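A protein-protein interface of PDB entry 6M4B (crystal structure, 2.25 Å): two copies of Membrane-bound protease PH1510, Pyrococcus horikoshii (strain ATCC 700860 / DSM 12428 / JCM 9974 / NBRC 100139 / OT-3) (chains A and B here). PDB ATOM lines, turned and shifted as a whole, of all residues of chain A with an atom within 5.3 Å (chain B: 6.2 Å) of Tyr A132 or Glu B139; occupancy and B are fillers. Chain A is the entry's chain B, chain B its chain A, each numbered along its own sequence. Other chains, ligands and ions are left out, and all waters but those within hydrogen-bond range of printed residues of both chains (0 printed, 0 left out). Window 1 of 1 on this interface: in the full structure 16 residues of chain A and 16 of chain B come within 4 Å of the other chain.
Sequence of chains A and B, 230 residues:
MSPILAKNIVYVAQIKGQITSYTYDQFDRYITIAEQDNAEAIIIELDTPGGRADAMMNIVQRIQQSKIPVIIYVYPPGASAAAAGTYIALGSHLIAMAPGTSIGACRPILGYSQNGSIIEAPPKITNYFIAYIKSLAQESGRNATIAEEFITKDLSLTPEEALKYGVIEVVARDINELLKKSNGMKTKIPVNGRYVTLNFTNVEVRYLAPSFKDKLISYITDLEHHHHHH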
ATOM      1  N   MET A  56      -8.072   8.144  17.489  1.00  0.00           N
ATOM      2  CA  MET A  56      -9.432   7.567  17.793  1.00  0.00           C
ATOM      3  C   MET A  56     -10.144   7.012  16.577  1.00  0.00           C
ATOM      4  O   MET A  56     -10.620   5.877  16.587  1.00  0.00           O
ATOM      5  CB  MET A  56     -10.292   8.618  18.520  1.00  0.00           C
ATOM      6  CG  MET A  56     -11.744   8.253  18.733  1.00  0.00           C
ATOM      7  SD  MET A  56     -12.851   8.681  17.368  1.00  0.00           S
ATOM      8  CE  MET A  56     -12.959  10.435  17.696  1.00  0.00           C
ATOM      9  N   MET A  57     -10.206   7.820  15.511  1.00  0.00           N
ATOM     10  CA  MET A  57     -10.872   7.401  14.265  1.00  0.00           C
ATOM     11  C   MET A  57     -10.232   6.171  13.657  1.00  0.00           C
ATOM     12  O   MET A  57     -10.951   5.270  13.252  1.00  0.00           O
ATOM     13  CB  MET A  57     -10.979   8.551  13.263  1.00  0.00           C
ATOM     14  CG  MET A  57     -12.065   9.544  13.630  1.00  0.00           C
ATOM     15  SD  MET A  57     -11.948  10.972  12.520  1.00  0.00           S
ATOM     16  CE  MET A  57     -12.827  12.187  13.452  1.00  0.00           C
ATOM     17  N   VAL A  60     -11.244   3.293  15.998  1.00  0.00           N
ATOM     18  CA  VAL A  60     -12.633   2.900  15.686  1.00  0.00           C
ATOM     19  C   VAL A  60     -12.707   2.051  14.428  1.00  0.00           C
ATOM     20  O   VAL A  60     -13.388   1.012  14.395  1.00  0.00           O
ATOM     21  CB  VAL A  60     -13.559   4.136  15.558  1.00  0.00           C
ATOM     22  CG1 VAL A  60     -14.848   3.775  14.893  1.00  0.00           C
ATOM     23  CG2 VAL A  60     -13.799   4.734  16.943  1.00  0.00           C
ATOM     24  N   TYR A  87     -15.888   7.185  22.002  1.00  0.00           N
ATOM     25  CA  TYR A  87     -16.091   6.833  20.590  1.00  0.00           C
ATOM     26  C   TYR A  87     -15.565   5.405  20.336  1.00  0.00           C
ATOM     27  O   TYR A  87     -16.173   4.652  19.626  1.00  0.00           O
ATOM     28  CB  TYR A  87     -15.385   7.835  19.662  1.00  0.00           C
ATOM     29  CG  TYR A  87     -15.863   9.278  19.622  1.00  0.00           C
ATOM     30  CD1 TYR A  87     -15.546  10.176  20.628  1.00  0.00           C
ATOM     31  CD2 TYR A  87     -16.588   9.762  18.557  1.00  0.00           C
ATOM     32  CE1 TYR A  87     -15.965  11.489  20.596  1.00  0.00           C
ATOM     33  CE2 TYR A  87     -16.974  11.102  18.501  1.00  0.00           C
ATOM     34  CZ  TYR A  87     -16.659  11.945  19.515  1.00  0.00           C
ATOM     35  OH  TYR A  87     -17.022  13.238  19.448  1.00  0.00           O
ATOM     36  N   ASN A 127     -20.372  20.137  15.079  1.00  0.00           N
ATOM     37  CA  ASN A 127     -21.423  19.402  14.379  1.00  0.00           C
ATOM     38  C   ASN A 127     -20.913  18.197  13.618  1.00  0.00           C
ATOM     39  O   ASN A 127     -21.611  17.201  13.498  1.00  0.00           O
ATOM     40  CB  ASN A 127     -22.218  20.288  13.436  1.00  0.00           C
ATOM     41  CG  ASN A 127     -23.052  21.317  14.172  1.00  0.00           C
ATOM     42  OD1 ASN A 127     -23.512  21.112  15.303  1.00  0.00           O
ATOM     43  ND2 ASN A 127     -23.303  22.417  13.508  1.00  0.00           N
ATOM     44  N   TYR A 128     -19.706  18.304  13.112  1.00  0.00           N
ATOM     45  CA  TYR A 128     -19.064  17.189  12.499  1.00  0.00           C
ATOM     46  C   TYR A 128     -18.940  16.002  13.488  1.00  0.00           C
ATOM     47  O   TYR A 128     -19.186  14.829  13.135  1.00  0.00           O
ATOM     48  CB  TYR A 128     -17.711  17.632  11.954  1.00  0.00           C
ATOM     49  CG  TYR A 128     -16.872  16.497  11.450  1.00  0.00           C
ATOM     50  CD1 TYR A 128     -16.007  15.793  12.310  1.00  0.00           C
ATOM     51  CD2 TYR A 128     -16.943  16.106  10.131  1.00  0.00           C
ATOM     52  CE1 TYR A 128     -15.251  14.725  11.860  1.00  0.00           C
ATOM     53  CE2 TYR A 128     -16.156  15.072   9.663  1.00  0.00           C
ATOM     54  CZ  TYR A 128     -15.344  14.368  10.528  1.00  0.00           C
ATOM     55  OH  TYR A 128     -14.618  13.310  10.059  1.00  0.00           O
ATOM     56  N   PHE A 129     -18.492  16.312  14.690  1.00  0.00           N
ATOM     57  CA  PHE A 129     -18.277  15.301  15.702  1.00  0.00           C
ATOM     58  C   PHE A 129     -19.590  14.722  16.182  1.00  0.00           C
ATOM     59  O   PHE A 129     -19.663  13.513  16.438  1.00  0.00           O
ATOM     60  CB  PHE A 129     -17.375  15.808  16.818  1.00  0.00           C
ATOM     61  CG  PHE A 129     -15.909  15.667  16.479  1.00  0.00           C
ATOM     62  CD1 PHE A 129     -15.344  14.431  16.432  1.00  0.00           C
ATOM     63  CD2 PHE A 129     -15.150  16.760  16.083  1.00  0.00           C
ATOM     64  CE1 PHE A 129     -14.002  14.256  16.058  1.00  0.00           C
ATOM     65  CE2 PHE A 129     -13.800  16.618  15.731  1.00  0.00           C
ATOM     66  CZ  PHE A 129     -13.213  15.367  15.763  1.00  0.00           C
ATOM     67  N   ILE A 130     -20.606  15.571  16.278  1.00  0.00           N
ATOM     68  CA  ILE A 130     -21.933  15.145  16.604  1.00  0.00           C
ATOM     69  C   ILE A 130     -22.419  14.160  15.542  1.00  0.00           C
ATOM     70  O   ILE A 130     -22.906  13.086  15.882  1.00  0.00           O
ATOM     71  CB  ILE A 130     -22.922  16.323  16.724  1.00  0.00           C
ATOM     72  CG1 ILE A 130     -22.585  17.176  17.956  1.00  0.00           C
ATOM     73  CG2 ILE A 130     -24.341  15.807  16.819  1.00  0.00           C
ATOM     74  CD1 ILE A 130     -23.312  18.483  18.069  1.00  0.00           C
ATOM     75  N   ALA A 131     -22.275  14.497  14.262  1.00  0.00           N
ATOM     76  CA  ALA A 131     -22.665  13.560  13.251  1.00  0.00           C
ATOM     77  C   ALA A 131     -21.906  12.232  13.422  1.00  0.00           C
ATOM     78  O   ALA A 131     -22.487  11.162  13.243  1.00  0.00           O
ATOM     79  CB  ALA A 131     -22.467  14.150  11.852  1.00  0.00           C
ATOM     80  N   TYR A 132     -20.631  12.283  13.733  1.00  0.00           N
ATOM     81  CA  TYR A 132     -19.823  11.063  13.810  1.00  0.00           C
ATOM     82  C   TYR A 132     -20.212  10.160  15.017  1.00  0.00           C
ATOM     83  O   TYR A 132     -20.477   8.965  14.845  1.00  0.00           O
ATOM     84  CB  TYR A 132     -18.351  11.392  13.836  1.00  0.00           C
ATOM     85  CG  TYR A 132     -17.424  10.219  13.862  1.00  0.00           C
ATOM     86  CD1 TYR A 132     -17.263   9.415  12.768  1.00  0.00           C
ATOM     87  CD2 TYR A 132     -16.618   9.981  14.962  1.00  0.00           C
ATOM     88  CE1 TYR A 132     -16.384   8.334  12.784  1.00  0.00           C
ATOM     89  CE2 TYR A 132     -15.769   8.898  15.015  1.00  0.00           C
ATOM     90  CZ  TYR A 132     -15.649   8.074  13.942  1.00  0.00           C
ATOM     91  OH  TYR A 132     -14.752   7.020  14.019  1.00  0.00           O
ATOM     92  N   ILE A 133     -20.354  10.780  16.184  1.00  0.00           N
ATOM     93  CA  ILE A 133     -20.707  10.054  17.406  1.00  0.00           C
ATOM     94  C   ILE A 133     -22.097   9.428  17.280  1.00  0.00           C
ATOM     95  O   ILE A 133     -22.313   8.280  17.685  1.00  0.00           O
ATOM     96  CB  ILE A 133     -20.515  10.907  18.704  1.00  0.00           C
ATOM     97  CG1 ILE A 133     -20.216   9.958  19.872  1.00  0.00           C
ATOM     98  CG2 ILE A 133     -21.728  11.815  18.968  1.00  0.00           C
ATOM     99  CD1 ILE A 133     -19.948  10.653  21.184  1.00  0.00           C
ATOM    100  N   LYS A 134     -23.006  10.142  16.622  1.00  0.00           N
ATOM    101  CA  LYS A 134     -24.353   9.646  16.446  1.00  0.00           C
ATOM    102  C   LYS A 134     -24.383   8.456  15.498  1.00  0.00           C
ATOM    103  O   LYS A 134     -25.163   7.542  15.667  1.00  0.00           O
ATOM    104  CB  LYS A 134     -25.279  10.737  15.964  1.00  0.00           C
ATOM    105  CG  LYS A 134     -25.756  11.672  17.069  1.00  0.00           C
ATOM    106  CD  LYS A 134     -26.608  12.815  16.537  1.00  0.00           C
ATOM    107  CE  LYS A 134     -27.966  12.394  16.014  1.00  0.00           C
ATOM    108  NZ  LYS A 134     -29.105  13.004  16.765  1.00  0.00           N
ATOM    109  N   SER A 135     -23.520   8.487  14.499  1.00  0.00           N
ATOM    110  CA  SER A 135     -23.442   7.427  13.551  1.00  0.00           C
ATOM    111  C   SER A 135     -22.934   6.169  14.239  1.00  0.00           C
ATOM    112  O   SER A 135     -23.454   5.107  13.943  1.00  0.00           O
ATOM    113  CB  SER A 135     -22.543   7.793  12.360  1.00  0.00           C
ATOM    114  OG  SER A 135     -21.144   7.801  12.701  1.00  0.00           O
ATOM    115  N   LEU A 136     -21.933   6.275  15.115  1.00  0.00           N
ATOM    116  CA  LEU A 136     -21.448   5.082  15.858  1.00  0.00           C
ATOM    117  C   LEU A 136     -22.580   4.498  16.696  1.00  0.00           C
ATOM    118  O   LEU A 136     -22.783   3.286  16.706  1.00  0.00           O
ATOM    119  CB  LEU A 136     -20.228   5.389  16.721  1.00  0.00           C
ATOM    120  CG  LEU A 136     -19.021   5.969  15.968  1.00  0.00           C
ATOM    121  CD1 LEU A 136     -17.906   6.202  16.965  1.00  0.00           C
ATOM    122  CD2 LEU A 136     -18.579   5.031  14.851  1.00  0.00           C
ATOM    123  N   ALA A 137     -23.379   5.368  17.319  1.00  0.00           N
ATOM    124  CA  ALA A 137     -24.539   4.925  18.100  1.00  0.00           C
ATOM    125  C   ALA A 137     -25.602   4.276  17.230  1.00  0.00           C
ATOM    126  O   ALA A 137     -26.053   3.166  17.555  1.00  0.00           O
ATOM    127  CB  ALA A 137     -25.148   6.054  18.922  1.00  0.00           C
ATOM    128  N   GLN B  61     -12.206   6.326   4.629  1.00  0.00           N
ATOM    129  CA  GLN B  61     -11.399   6.729   5.774  1.00  0.00           C
ATOM    130  C   GLN B  61     -10.029   7.288   5.335  1.00  0.00           C
ATOM    131  O   GLN B  61      -9.483   8.168   5.977  1.00  0.00           O
ATOM    132  CB  GLN B  61     -11.222   5.584   6.788  1.00  0.00           C
ATOM    133  CG  GLN B  61     -11.424   6.066   8.240  1.00  0.00           C
ATOM    134  CD  GLN B  61     -10.255   5.800   9.116  1.00  0.00           C
ATOM    135  OE1 GLN B  61      -9.154   5.560   8.629  1.00  0.00           O
ATOM    136  NE2 GLN B  61     -10.464   5.876  10.412  1.00  0.00           N
ATOM    137  N   GLN B  64     -10.785  10.809   4.469  1.00  0.00           N
ATOM    138  CA  GLN B  64     -11.048  11.619   5.631  1.00  0.00           C
ATOM    139  C   GLN B  64      -9.793  12.036   6.387  1.00  0.00           C
ATOM    140  O   GLN B  64      -9.801  13.081   7.003  1.00  0.00           O
ATOM    141  CB  GLN B  64     -12.018  10.916   6.587  1.00  0.00           C
ATOM    142  CG  GLN B  64     -13.467  10.894   6.091  1.00  0.00           C
ATOM    143  CD  GLN B  64     -14.384  10.110   7.034  1.00  0.00           C
ATOM    144  OE1 GLN B  64     -13.952   9.128   7.662  1.00  0.00           O
ATOM    145  NE2 GLN B  64     -15.647  10.526   7.136  1.00  0.00           N
ATOM    146  N   LYS B 134     -25.807   8.380   5.881  1.00  0.00           N
ATOM    147  CA  LYS B 134     -26.328   9.598   6.466  1.00  0.00           C
ATOM    148  C   LYS B 134     -25.277  10.375   7.242  1.00  0.00           C
ATOM    149  O   LYS B 134     -25.248  11.604   7.206  1.00  0.00           O
ATOM    150  CB  LYS B 134     -27.529   9.321   7.346  1.00  0.00           C
ATOM    151  CG  LYS B 134     -28.808   9.084   6.565  1.00  0.00           C
ATOM    152  CD  LYS B 134     -29.973   8.723   7.464  1.00  0.00           C
ATOM    153  CE  LYS B 134     -30.457   9.871   8.348  1.00  0.00           C
ATOM    154  NZ  LYS B 134     -31.846  10.261   8.047  1.00  0.00           N
ATOM    155  N   SER B 135     -24.390   9.662   7.901  1.00  0.00           N
ATOM    156  CA  SER B 135     -23.325  10.265   8.612  1.00  0.00           C
ATOM    157  C   SER B 135     -22.342  10.965   7.655  1.00  0.00           C
ATOM    158  O   SER B 135     -21.906  12.042   7.985  1.00  0.00           O
ATOM    159  CB  SER B 135     -22.579   9.238   9.457  1.00  0.00           C
ATOM    160  OG  SER B 135     -21.733   8.371   8.719  1.00  0.00           O
ATOM    161  N   LEU B 136     -22.005  10.347   6.509  1.00  0.00           N
ATOM    162  CA  LEU B 136     -21.139  10.985   5.538  1.00  0.00           C
ATOM    163  C   LEU B 136     -21.805  12.277   5.011  1.00  0.00           C
ATOM    164  O   LEU B 136     -21.151  13.307   4.954  1.00  0.00           O
ATOM    165  CB  LEU B 136     -20.773  10.043   4.394  1.00  0.00           C
ATOM    166  CG  LEU B 136     -20.087   8.717   4.774  1.00  0.00           C
ATOM    167  CD1 LEU B 136     -19.780   7.967   3.510  1.00  0.00           C
ATOM    168  CD2 LEU B 136     -18.822   9.006   5.559  1.00  0.00           C
ATOM    169  N   ALA B 137     -23.113  12.236   4.760  1.00  0.00           N
ATOM    170  CA  ALA B 137     -23.834  13.426   4.395  1.00  0.00           C
ATOM    171  C   ALA B 137     -23.823  14.506   5.477  1.00  0.00           C
ATOM    172  O   ALA B 137     -23.527  15.657   5.186  1.00  0.00           O
ATOM    173  CB  ALA B 137     -25.273  13.096   3.981  1.00  0.00           C
ATOM    174  N   GLN B 138     -24.130  14.138   6.717  1.00  0.00           N
ATOM    175  CA  GLN B 138     -24.200  15.110   7.811  1.00  0.00           C
ATOM    176  C   GLN B 138     -22.841  15.682   8.099  1.00  0.00           C
ATOM    177  O   GLN B 138     -22.730  16.847   8.365  1.00  0.00           O
ATOM    178  CB  GLN B 138     -24.784  14.523   9.107  1.00  0.00           C
ATOM    179  CG  GLN B 138     -26.135  13.875   8.920  1.00  0.00           C
ATOM    180  CD  GLN B 138     -27.271  14.782   9.264  1.00  0.00           C
ATOM    181  OE1 GLN B 138     -27.106  16.021   9.335  1.00  0.00           O
ATOM    182  NE2 GLN B 138     -28.465  14.177   9.467  1.00  0.00           N
ATOM    183  N   GLU B 139     -21.816  14.848   8.078  1.00  0.00           N
ATOM    184  CA  GLU B 139     -20.464  15.308   8.310  1.00  0.00           C
ATOM    185  C   GLU B 139     -20.010  16.366   7.269  1.00  0.00           C
ATOM    186  O   GLU B 139     -19.194  17.206   7.584  1.00  0.00           O
ATOM    187  CB  GLU B 139     -19.484  14.125   8.262  1.00  0.00           C
ATOM    188  CG  GLU B 139     -19.538  13.291   9.531  1.00  0.00           C
ATOM    189  CD  GLU B 139     -18.977  11.883   9.377  1.00  0.00           C
ATOM    190  OE1 GLU B 139     -18.357  11.579   8.321  1.00  0.00           O
ATOM    191  OE2 GLU B 139     -19.180  11.076  10.324  1.00  0.00           O
ATOM    192  N   SER B 140     -20.492  16.254   6.040  1.00  0.00           N
ATOM    193  CA  SER B 140     -20.122  17.161   4.978  1.00  0.00           C
ATOM    194  C   SER B 140     -21.171  18.225   4.647  1.00  0.00           C
ATOM    195  O   SER B 140     -21.050  18.894   3.624  1.00  0.00           O
ATOM    196  CB  SER B 140     -19.820  16.333   3.736  1.00  0.00           C
ATOM    197  OG  SER B 140     -20.935  15.577   3.317  1.00  0.00           O
ATOM    198  N   GLY B 141     -22.210  18.391   5.485  1.00  0.00           N
ATOM    199  CA  GLY B 141     -23.237  19.399   5.205  1.00  0.00           C
ATOM    200  C   GLY B 141     -24.069  19.085   3.970  1.00  0.00           C
ATOM    201  O   GLY B 141     -24.737  19.926   3.476  1.00  0.00           O
ATOM    202  N   ARG B 142     -24.083  17.848   3.507  1.00  0.00           N
ATOM    203  CA  ARG B 142     -24.818  17.472   2.345  1.00  0.00           C
ATOM    204  C   ARG B 142     -26.173  16.859   2.742  1.00  0.00           C
ATOM    205  O   ARG B 142     -26.407  16.533   3.880  1.00  0.00           O
ATOM    206  CB  ARG B 142     -23.971  16.485   1.509  1.00  0.00           C
ATOM    207  CG  ARG B 142     -22.737  17.149   0.874  1.00  0.00           C
ATOM    208  CD  ARG B 142     -21.824  16.117   0.248  1.00  0.00           C
ATOM    209  NE  ARG B 142     -20.644  16.754  -0.267  1.00  0.00           N
ATOM    210  CZ  ARG B 142     -19.375  16.415  -0.039  1.00  0.00           C
ATOM    211  NH1 ARG B 142     -19.023  15.402   0.742  1.00  0.00           N
ATOM    212  NH2 ARG B 142     -18.425  17.117  -0.635  1.00  0.00           N
ATOM    213  N   LYS B 188     -15.872  20.567   2.326  1.00  0.00           N
ATOM    214  CA  LYS B 188     -17.092  20.280   3.049  1.00  0.00           C
ATOM    215  C   LYS B 188     -16.850  19.469   4.310  1.00  0.00           C
ATOM    216  O   LYS B 188     -17.697  19.415   5.170  1.00  0.00           O
ATOM    217  CB  LYS B 188     -18.118  19.551   2.148  1.00  0.00           C
ATOM    218  CG  LYS B 188     -18.669  20.360   0.982  1.00  0.00           C
ATOM    219  CD  LYS B 188     -19.139  21.781   1.260  1.00  0.00           C
ATOM    220  CE  LYS B 188     -20.226  21.949   2.310  1.00  0.00           C
ATOM    221  NZ  LYS B 188     -21.536  21.491   1.822  1.00  0.00           N
ATOM    222  N   ILE B 189     -15.697  18.838   4.405  1.00  0.00           N
ATOM    223  CA  ILE B 189     -15.263  18.153   5.614  1.00  0.00           C
ATOM    224  C   ILE B 189     -13.886  18.757   5.968  1.00  0.00           C
ATOM    225  O   ILE B 189     -13.224  19.352   5.124  1.00  0.00           O
ATOM    226  CB  ILE B 189     -15.163  16.610   5.449  1.00  0.00           C
ATOM    227  CG1 ILE B 189     -14.216  16.213   4.318  1.00  0.00           C
ATOM    228  CG2 ILE B 189     -16.518  16.007   5.192  1.00  0.00           C
ATOM    229  CD1 ILE B 189     -13.926  14.713   4.231  1.00  0.00           C
ATOM    230  N   PRO B 190     -13.470  18.652   7.221  1.00  0.00           N
ATOM    231  CA  PRO B 190     -12.173  19.217   7.603  1.00  0.00           C
ATOM    232  C   PRO B 190     -10.966  18.525   6.944  1.00  0.00           C
ATOM    233  O   PRO B 190     -11.046  17.376   6.509  1.00  0.00           O
ATOM    234  CB  PRO B 190     -12.129  19.017   9.146  1.00  0.00           C
ATOM    235  CG  PRO B 190     -13.501  18.623   9.547  1.00  0.00           C
ATOM    236  CD  PRO B 190     -14.137  17.977   8.347  1.00  0.00           C
ATOM    237  N   TYR B 195     -11.563  23.679   7.923  1.00  0.00           N
ATOM    238  CA  TYR B 195     -12.212  23.761   6.652  1.00  0.00           C
ATOM    239  C   TYR B 195     -11.429  24.718   5.735  1.00  0.00           C
ATOM    240  O   TYR B 195     -11.682  25.920   5.718  1.00  0.00           O
ATOM    241  CB  TYR B 195     -13.656  24.184   6.836  1.00  0.00           C
ATOM    242  CG  TYR B 195     -14.473  23.215   7.650  1.00  0.00           C
ATOM    243  CD1 TYR B 195     -15.192  22.176   7.030  1.00  0.00           C
ATOM    244  CD2 TYR B 195     -14.568  23.345   9.032  1.00  0.00           C
ATOM    245  CE1 TYR B 195     -15.967  21.282   7.757  1.00  0.00           C
ATOM    246  CE2 TYR B 195     -15.372  22.482   9.768  1.00  0.00           C
ATOM    247  CZ  TYR B 195     -16.048  21.433   9.112  1.00  0.00           C
ATOM    248  OH  TYR B 195     -16.781  20.569   9.817  1.00  0.00           O
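NE2 of Gln B61 lies within hydrogen-bond range of O of Met A57, 2.9 Å away.
The side-chain carboxylate (OE1) of Glu B139 lies within hydrogen-bond range of the side-chain amide nitrogen (NE2) of Gln B64. The side-chain hydroxyl (OG) of Ser A135 is in hydrogen-bond range of the backbone carbonyl oxygen (O) of Tyr A132 (2.5 Å).
Glu B139 touches Tyr A128. Tyr A128 touches Pro B190. Tyr A128 touches Tyr B195. Ala A131 touches Gln B138. CB of Ala A131 touches CG of Glu B139 (3.8 Å). Tyr A132 touches Glu B139. CB of Ser A135 touches CB of Ser B135, at 3.2 Å.
Printed residues of chain B within 4 Å of Tyr A132: Glu B139. Of the printed residues of chain A, Ser B135 touches Ser A135 (3.2 Å). Of the printed residues of chain A, Tyr B195 touches Tyr A128 (3.7 Å). The nearest residue of chain A that does not touch Glu B139 is Ser A135 (4.5 Å). The nearest printed residue of chain A that does not touch Gln B61 is Tyr A132 (5.7 Å).
Printed residues of chain B that touch a printed residue of chain A: Gln B61, Ser B135, Gln B138, Glu B139, Pro B190 and Tyr B195. Printed residues of chain A that touch a printed residue of chain B: Met A57, Tyr A128, Ala A131, Tyr A132 and Ser A135. Among the printed residues, no Asp or Glu carboxylate lies within 4 Å of a Lys or Arg side-chain nitrogen of the other chain.
Ser A135 touches its own counterpart, Ser B135. Positions printed for both chains: 134, 135, 136 and 137.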
